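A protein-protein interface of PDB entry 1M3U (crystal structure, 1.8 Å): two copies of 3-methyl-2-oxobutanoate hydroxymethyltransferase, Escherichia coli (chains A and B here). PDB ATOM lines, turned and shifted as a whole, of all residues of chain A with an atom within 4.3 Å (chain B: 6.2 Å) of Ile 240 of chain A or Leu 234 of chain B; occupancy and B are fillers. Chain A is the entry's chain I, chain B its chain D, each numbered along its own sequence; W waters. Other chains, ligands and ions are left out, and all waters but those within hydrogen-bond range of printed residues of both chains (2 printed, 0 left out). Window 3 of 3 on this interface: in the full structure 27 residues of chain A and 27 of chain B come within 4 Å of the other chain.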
ATOM      1  N   LEU A  32     -11.167   2.709  13.683  1.00  0.00           N
ATOM      2  CA  LEU A  32     -10.391   1.939  14.632  1.00  0.00           C
ATOM      3  C   LEU A  32      -9.445   2.825  15.424  1.00  0.00           C
ATOM      4  O   LEU A  32      -9.418   2.761  16.645  1.00  0.00           O
ATOM      5  CB  LEU A  32      -9.603   0.857  13.903  1.00  0.00           C
ATOM      6  CG  LEU A  32      -8.852  -0.211  14.697  1.00  0.00           C
ATOM      7  CD1 LEU A  32      -8.669  -1.458  13.772  1.00  0.00           C
ATOM      8  CD2 LEU A  32      -7.505   0.282  15.269  1.00  0.00           C
ATOM      9  N   LEU A 234       1.928  -4.958  15.529  1.00  0.00           N
ATOM     10  CA  LEU A 234       1.043  -6.107  15.571  1.00  0.00           C
ATOM     11  C   LEU A 234       1.749  -7.396  16.005  1.00  0.00           C
ATOM     12  O   LEU A 234       1.176  -8.201  16.751  1.00  0.00           O
ATOM     13  CB  LEU A 234       0.378  -6.294  14.220  1.00  0.00           C
ATOM     14  CG  LEU A 234      -0.573  -7.471  14.111  1.00  0.00           C
ATOM     15  CD1 LEU A 234      -1.728  -7.314  15.088  1.00  0.00           C
ATOM     16  CD2 LEU A 234      -1.067  -7.562  12.709  1.00  0.00           C
ATOM     17  N   GLY A 238      -0.705  -8.995  18.949  1.00  0.00           N
ATOM     18  CA  GLY A 238      -1.670  -9.991  18.527  1.00  0.00           C
ATOM     19  C   GLY A 238      -2.889  -9.507  17.766  1.00  0.00           C
ATOM     20  O   GLY A 238      -3.406 -10.226  16.916  1.00  0.00           O
ATOM     21  N   ASP A 239      -3.385  -8.322  18.099  1.00  0.00           N
ATOM     22  CA  ASP A 239      -4.584  -7.779  17.454  1.00  0.00           C
ATOM     23  C   ASP A 239      -4.369  -6.294  17.186  1.00  0.00           C
ATOM     24  O   ASP A 239      -3.556  -5.651  17.855  1.00  0.00           O
ATOM     25  CB  ASP A 239      -5.842  -8.020  18.303  1.00  0.00           C
ATOM     26  CG  ASP A 239      -5.827  -7.257  19.619  1.00  0.00           C
ATOM     27  OD1 ASP A 239      -6.110  -6.031  19.631  1.00  0.00           O
ATOM     28  OD2 ASP A 239      -5.562  -7.812  20.698  1.00  0.00           O
ATOM     29  N   ILE A 240      -5.082  -5.747  16.211  1.00  0.00           N
ATOM     30  CA  ILE A 240      -4.691  -4.430  15.682  1.00  0.00           C
ATOM     31  C   ILE A 240      -4.952  -3.326  16.703  1.00  0.00           C
ATOM     32  O   ILE A 240      -4.160  -2.396  16.817  1.00  0.00           O
ATOM     33  CB  ILE A 240      -5.377  -4.158  14.286  1.00  0.00           C
ATOM     34  CG1 ILE A 240      -4.852  -5.163  13.243  1.00  0.00           C
ATOM     35  CG2 ILE A 240      -5.178  -2.718  13.805  1.00  0.00           C
ATOM     36  CD1 ILE A 240      -5.654  -5.228  11.958  1.00  0.00           C
ATOM     37  N   ARG A 241      -6.064  -3.420  17.424  1.00  0.00           N
ATOM     38  CA  ARG A 241      -6.360  -2.426  18.456  1.00  0.00           C
ATOM     39  C   ARG A 241      -5.325  -2.399  19.547  1.00  0.00           C
ATOM     40  O   ARG A 241      -4.958  -1.320  19.985  1.00  0.00           O
ATOM     41  CB  ARG A 241      -7.754  -2.599  19.038  1.00  0.00           C
ATOM     42  CG  ARG A 241      -8.833  -2.166  18.048  1.00  0.00           C
ATOM     43  CD  ARG A 241     -10.248  -2.624  18.389  1.00  0.00           C
ATOM     44  NE  ARG A 241     -11.211  -2.086  17.414  1.00  0.00           N
ATOM     45  CZ  ARG A 241     -11.417  -2.588  16.211  1.00  0.00           C
ATOM     46  NH1 ARG A 241     -10.741  -3.645  15.783  1.00  0.00           N
ATOM     47  NH2 ARG A 241     -12.295  -2.021  15.418  1.00  0.00           N
ATOM     48  N   ALA A 242      -4.821  -3.556  19.964  1.00  0.00           N
ATOM     49  CA  ALA A 242      -3.747  -3.618  20.949  1.00  0.00           C
ATOM     50  C   ALA A 242      -2.447  -3.065  20.400  1.00  0.00           C
ATOM     51  O   ALA A 242      -1.654  -2.469  21.149  1.00  0.00           O
ATOM     52  CB  ALA A 242      -3.527  -5.048  21.456  1.00  0.00           C
ATOM     53  N   ALA A 243      -2.202  -3.306  19.114  1.00  0.00           N
ATOM     54  CA  ALA A 243      -1.014  -2.772  18.445  1.00  0.00           C
ATOM     55  C   ALA A 243      -1.062  -1.249  18.450  1.00  0.00           C
ATOM     56  O   ALA A 243      -0.048  -0.611  18.695  1.00  0.00           O
ATOM     57  CB  ALA A 243      -0.920  -3.316  17.014  1.00  0.00           C
ATOM     58  N   VAL A 244      -2.243  -0.682  18.173  1.00  0.00           N
ATOM     59  CA  VAL A 244      -2.469   0.774  18.206  1.00  0.00           C
ATOM     60  C   VAL A 244      -2.150   1.339  19.600  1.00  0.00           C
ATOM     61  O   VAL A 244      -1.424   2.327  19.747  1.00  0.00           O
ATOM     62  CB  VAL A 244      -3.911   1.117  17.788  1.00  0.00           C
ATOM     63  CG1 VAL A 244      -4.284   2.578  18.076  1.00  0.00           C
ATOM     64  CG2 VAL A 244      -4.125   0.865  16.259  1.00  0.00           C
ATOM     65  N   ALA B 218     -12.307 -10.234   8.287  1.00  0.00           N
ATOM     66  CA  ALA B 218     -11.317 -11.305   8.417  1.00  0.00           C
ATOM     67  C   ALA B 218     -10.171 -10.985   9.354  1.00  0.00           C
ATOM     68  O   ALA B 218      -9.650 -11.909  10.011  1.00  0.00           O
ATOM     69  CB  ALA B 218     -10.789 -11.691   7.069  1.00  0.00           C
ATOM     70  N   PHE B 219      -9.760  -9.711   9.461  1.00  0.00           N
ATOM     71  CA  PHE B 219      -8.712  -9.311  10.425  1.00  0.00           C
ATOM     72  C   PHE B 219      -9.147  -8.441  11.571  1.00  0.00           C
ATOM     73  O   PHE B 219      -8.347  -7.751  12.212  1.00  0.00           O
ATOM     74  CB  PHE B 219      -7.532  -8.721   9.687  1.00  0.00           C
ATOM     75  CG  PHE B 219      -7.261  -9.463   8.388  1.00  0.00           C
ATOM     76  CD1 PHE B 219      -7.158 -10.848   8.383  1.00  0.00           C
ATOM     77  CD2 PHE B 219      -7.154  -8.791   7.204  1.00  0.00           C
ATOM     78  CE1 PHE B 219      -6.929 -11.547   7.209  1.00  0.00           C
ATOM     79  CE2 PHE B 219      -6.941  -9.482   6.007  1.00  0.00           C
ATOM     80  CZ  PHE B 219      -6.841 -10.850   6.005  1.00  0.00           C
ATOM     81  N   GLY B 220     -10.417  -8.528  11.898  1.00  0.00           N
ATOM     82  CA  GLY B 220     -10.942  -7.781  13.027  1.00  0.00           C
ATOM     83  C   GLY B 220     -10.745  -6.280  12.914  1.00  0.00           C
ATOM     84  O   GLY B 220     -10.668  -5.587  13.926  1.00  0.00           O
ATOM     85  N   ILE B 221     -10.679  -5.758  11.685  1.00  0.00           N
ATOM     86  CA  ILE B 221     -10.535  -4.304  11.504  1.00  0.00           C
ATOM     87  C   ILE B 221     -11.859  -3.618  11.797  1.00  0.00           C
ATOM     88  O   ILE B 221     -11.937  -2.571  12.463  1.00  0.00           O
ATOM     89  CB  ILE B 221     -10.067  -3.986  10.079  1.00  0.00           C
ATOM     90  CG1 ILE B 221      -8.696  -4.629   9.829  1.00  0.00           C
ATOM     91  CG2 ILE B 221     -10.009  -2.472   9.902  1.00  0.00           C
ATOM     92  CD1 ILE B 221      -8.425  -4.950   8.434  1.00  0.00           C
ATOM     93  N   LYS B 231     -15.692 -14.691  10.046  1.00  0.00           N
ATOM     94  CA  LYS B 231     -14.745 -15.150  11.042  1.00  0.00           C
ATOM     95  C   LYS B 231     -13.519 -14.242  11.038  1.00  0.00           C
ATOM     96  O   LYS B 231     -12.969 -13.961   9.995  1.00  0.00           O
ATOM     97  CB  LYS B 231     -14.341 -16.618  10.803  1.00  0.00           C
ATOM     98  CG  LYS B 231     -13.302 -17.137  11.751  1.00  0.00           C
ATOM     99  CD  LYS B 231     -13.073 -18.614  11.570  1.00  0.00           C
ATOM    100  CE  LYS B 231     -11.969 -19.171  12.470  1.00  0.00           C
ATOM    101  NZ  LYS B 231     -11.914 -20.670  12.385  1.00  0.00           N
ATOM    102  N   ASN B 232     -13.133 -13.805  12.236  1.00  0.00           N
ATOM    103  CA  ASN B 232     -11.878 -13.103  12.467  1.00  0.00           C
ATOM    104  C   ASN B 232     -10.756 -14.166  12.564  1.00  0.00           C
ATOM    105  O   ASN B 232     -10.591 -14.807  13.567  1.00  0.00           O
ATOM    106  CB  ASN B 232     -11.963 -12.254  13.764  1.00  0.00           C
ATOM    107  CG  ASN B 232     -10.672 -11.496  14.051  1.00  0.00           C
ATOM    108  OD1 ASN B 232      -9.706 -11.673  13.329  1.00  0.00           O
ATOM    109  ND2 ASN B 232     -10.643 -10.661  15.111  1.00  0.00           N
ATOM    110  N   PHE B 233     -10.010 -14.336  11.485  1.00  0.00           N
ATOM    111  CA  PHE B 233      -8.887 -15.268  11.453  1.00  0.00           C
ATOM    112  C   PHE B 233      -7.601 -14.701  12.105  1.00  0.00           C
ATOM    113  O   PHE B 233      -6.724 -15.446  12.495  1.00  0.00           O
ATOM    114  CB  PHE B 233      -8.612 -15.652   9.987  1.00  0.00           C
ATOM    115  CG  PHE B 233      -9.628 -16.594   9.407  1.00  0.00           C
ATOM    116  CD1 PHE B 233     -10.757 -16.125   8.753  1.00  0.00           C
ATOM    117  CD2 PHE B 233      -9.448 -17.956   9.530  1.00  0.00           C
ATOM    118  CE1 PHE B 233     -11.702 -17.007   8.224  1.00  0.00           C
ATOM    119  CE2 PHE B 233     -10.378 -18.830   9.014  1.00  0.00           C
ATOM    120  CZ  PHE B 233     -11.496 -18.339   8.354  1.00  0.00           C
ATOM    121  N   LEU B 234      -7.482 -13.389  12.200  1.00  0.00           N
ATOM    122  CA  LEU B 234      -6.330 -12.781  12.865  1.00  0.00           C
ATOM    123  C   LEU B 234      -6.278 -13.122  14.341  1.00  0.00           C
ATOM    124  O   LEU B 234      -5.207 -13.408  14.885  1.00  0.00           O
ATOM    125  CB  LEU B 234      -6.350 -11.250  12.669  1.00  0.00           C
ATOM    126  CG  LEU B 234      -5.210 -10.487  13.313  1.00  0.00           C
ATOM    127  CD1 LEU B 234      -3.881 -11.100  12.844  1.00  0.00           C
ATOM    128  CD2 LEU B 234      -5.281  -9.069  13.015  1.00  0.00           C
ATOM    129  N   ALA B 235      -7.423 -13.179  15.010  1.00  0.00           N
ATOM    130  CA  ALA B 235      -7.451 -13.479  16.448  1.00  0.00           C
ATOM    131  C   ALA B 235      -6.539 -14.650  16.907  1.00  0.00           C
ATOM    132  O   ALA B 235      -5.872 -14.580  17.958  1.00  0.00           O
ATOM    133  CB  ALA B 235      -8.894 -13.752  16.888  1.00  0.00           C
ATOM    134  N   GLU B 236      -6.509 -15.742  16.155  1.00  0.00           N
ATOM    135  CA  GLU B 236      -5.876 -16.952  16.693  1.00  0.00           C
ATOM    136  C   GLU B 236      -4.744 -17.471  15.831  1.00  0.00           C
ATOM    137  O   GLU B 236      -4.404 -18.653  15.926  1.00  0.00           O
ATOM    138  CB  GLU B 236      -6.905 -18.048  16.889  1.00  0.00           C
ATOM    139  CG  GLU B 236      -8.331 -17.546  17.067  1.00  0.00           C
ATOM    140  CD  GLU B 236      -9.327 -18.675  17.074  1.00  0.00           C
ATOM    141  OE1 GLU B 236      -9.066 -19.636  17.809  1.00  0.00           O
ATOM    142  OE2 GLU B 236     -10.348 -18.601  16.342  1.00  0.00           O
ATOM    143  N   THR B 237      -4.201 -16.591  14.976  1.00  0.00           N
ATOM    144  CA  THR B 237      -2.944 -16.835  14.249  1.00  0.00           C
ATOM    145  C   THR B 237      -1.854 -15.809  14.587  1.00  0.00           C
ATOM    146  O   THR B 237      -0.655 -16.108  14.469  1.00  0.00           O
ATOM    147  CB  THR B 237      -3.154 -16.850  12.729  1.00  0.00           C
ATOM    148  OG1 THR B 237      -3.845 -15.673  12.319  1.00  0.00           O
ATOM    149  CG2 THR B 237      -4.048 -17.995  12.341  1.00  0.00           C
ATOM    150  N   GLY B 238      -2.262 -14.619  15.012  1.00  0.00           N
ATOM    151  CA  GLY B 238      -1.317 -13.634  15.506  1.00  0.00           C
ATOM    152  C   GLY B 238      -0.842 -12.604  14.492  1.00  0.00           C
ATOM    153  O   GLY B 238      -0.645 -11.449  14.850  1.00  0.00           O
ATOM    154  N   ASP B 239      -0.636 -13.019  13.240  1.00  0.00           N
ATOM    155  CA  ASP B 239      -0.240 -12.109  12.172  1.00  0.00           C
ATOM    156  C   ASP B 239      -1.064 -12.336  10.903  1.00  0.00           C
ATOM    157  O   ASP B 239      -1.561 -13.440  10.657  1.00  0.00           O
ATOM    158  CB  ASP B 239       1.252 -12.225  11.845  1.00  0.00           C
ATOM    159  CG  ASP B 239       1.628 -13.581  11.253  1.00  0.00           C
ATOM    160  OD1 ASP B 239       1.938 -14.501  12.038  1.00  0.00           O
ATOM    161  OD2 ASP B 239       1.665 -13.800  10.011  1.00  0.00           O
ATOM    162  N   ILE B 240      -1.182 -11.289  10.108  1.00  0.00           N
ATOM    163  CA  ILE B 240      -2.124 -11.252   8.991  1.00  0.00           C
ATOM    164  C   ILE B 240      -1.876 -12.345   7.934  1.00  0.00           C
ATOM    165  O   ILE B 240      -2.824 -12.976   7.494  1.00  0.00           O
ATOM    166  CB  ILE B 240      -2.210  -9.866   8.378  1.00  0.00           C
ATOM    167  CG1 ILE B 240      -2.742  -8.854   9.426  1.00  0.00           C
ATOM    168  CG2 ILE B 240      -3.107  -9.881   7.100  1.00  0.00           C
ATOM    169  CD1 ILE B 240      -2.410  -7.400   9.116  1.00  0.00           C
ATOM    170  N   ALA B 243      -3.050 -15.626   9.198  1.00  0.00           N
ATOM    171  CA  ALA B 243      -4.528 -15.567   9.144  1.00  0.00           C
ATOM    172  C   ALA B 243      -5.064 -15.874   7.754  1.00  0.00           C
ATOM    173  O   ALA B 243      -6.018 -16.606   7.631  1.00  0.00           O
ATOM    174  CB  ALA B 243      -5.037 -14.208   9.593  1.00  0.00           C
HETATM  175  O   HOH W   1     -11.845  -6.822  16.282  1.00  0.00           O
HETATM  176  O   HOH W   2      -7.594  -7.060  15.039  1.00  0.00           O
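The backbone carbonyl oxygen of Gly 220 of chain B lies within hydrogen-bond range of the guanidinium group of Arg 241 of chain A, at 2.7 Å.
NH2 of Arg 241 of chain A is in hydrogen-bond range of O of Ile 221 of chain B (3.0 Å).
The backbone NH (N) of Arg 241 of chain A sits close to the side-chain carboxylate (OD1) of Asp 239 of chain A (3.4 Å).
The backbone carbonyl oxygen (O) of Ala 218 of chain B is in hydrogen-bond range of the backbone NH (N) of Leu 234 of chain B.
The backbone NH (N) of Leu 234 of chain B lies within hydrogen-bond range of the side-chain amide oxygen (OD1) of Asn 232 of chain B (3.0 Å).
CD1 of Leu 32 of chain A touches O of Ile 221 of chain B, 3.7 Å away.
Leu 234 of chain A touches Ile 240 of chain B (CD2 to CD1, 3.8 Å).
Gly 238 of chain A touches Gly 238 of chain B (O to O, 3.7 Å).
CD1 of Ile 240 of chain A touches O of Phe 219 of chain B, 3.7 Å away.
Ile 240 of chain A touches Ile 221 of chain B.
Ile 240 of chain A touches Leu 234 of chain B.
Of the printed residues of chain B, Leu 234 of chain A touches Ile 240.
Of the printed residues of chain B, Ile 240 of chain A touches Phe 219, Ile 221 and Leu 234.
Val 244 of chain A touches none of the printed residues of chain B.
Printed residues of chain A within 4 Å of Phe 219 of chain B: Ile 240.
Of the printed residues of chain A, Ile 221 of chain B touches Leu 32, Ile 240 and Arg 241.
Of the printed residues of chain A, Leu 234 of chain B touches Ile 240 (3.9 Å).
Of the printed residues of chain A, Gly 238 of chain B touches Gly 238 (3.7 Å).
The nearest printed residue of chain B that does not touch Ile 240 of chain A is Ile 240 of chain B (4.8 Å).
The nearest printed residue of chain A that does not touch Leu 234 of chain B is Gly 238 of chain A (4.04 Å).
The nearest printed residue of chain A that does not touch Ile 221 of chain B is Asp 239 of chain A (8.4 Å).
Of the 15 printed residues of chain B, 6 touch a printed residue of chain A.
Hydrophobic or aromatic side chains of chain B that line the printed part of chain A: Ile 221, Leu 234 and Ile 240.
Of the 9 printed residues of chain A, 5 touch a printed residue of chain B.
Among the printed residues, 8 pairs touch across the chains.
Among the printed residues, no Asp or Glu carboxylate lies within 4 Å of a Lys or Arg side-chain nitrogen of the other chain.
Leu 234 of chain A touches Ile 240 of chain B, and with the chains exchanged Ile 240 of chain A touches Leu 234 of chain B.
Gly 238 of chain A touches its own counterpart, Gly 238 of chain B.
5 positions are printed for both chains.
Of the 8 pairs that touch across the chains among the printed residues, 3 have their exchanged pair printed and touching as well.
Water W1 lies within hydrogen-bond range of O of Gly 220 of chain B (2.9 Å) and NH1 of Arg 241 of chain A (3.4 Å).
Water W2 lies within hydrogen-bond range of the backbone carbonyl oxygen (O) of Phe 219 of chain B (3.0 Å) and the backbone NH (N) of Ile 240 of chain A (3.1 Å).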
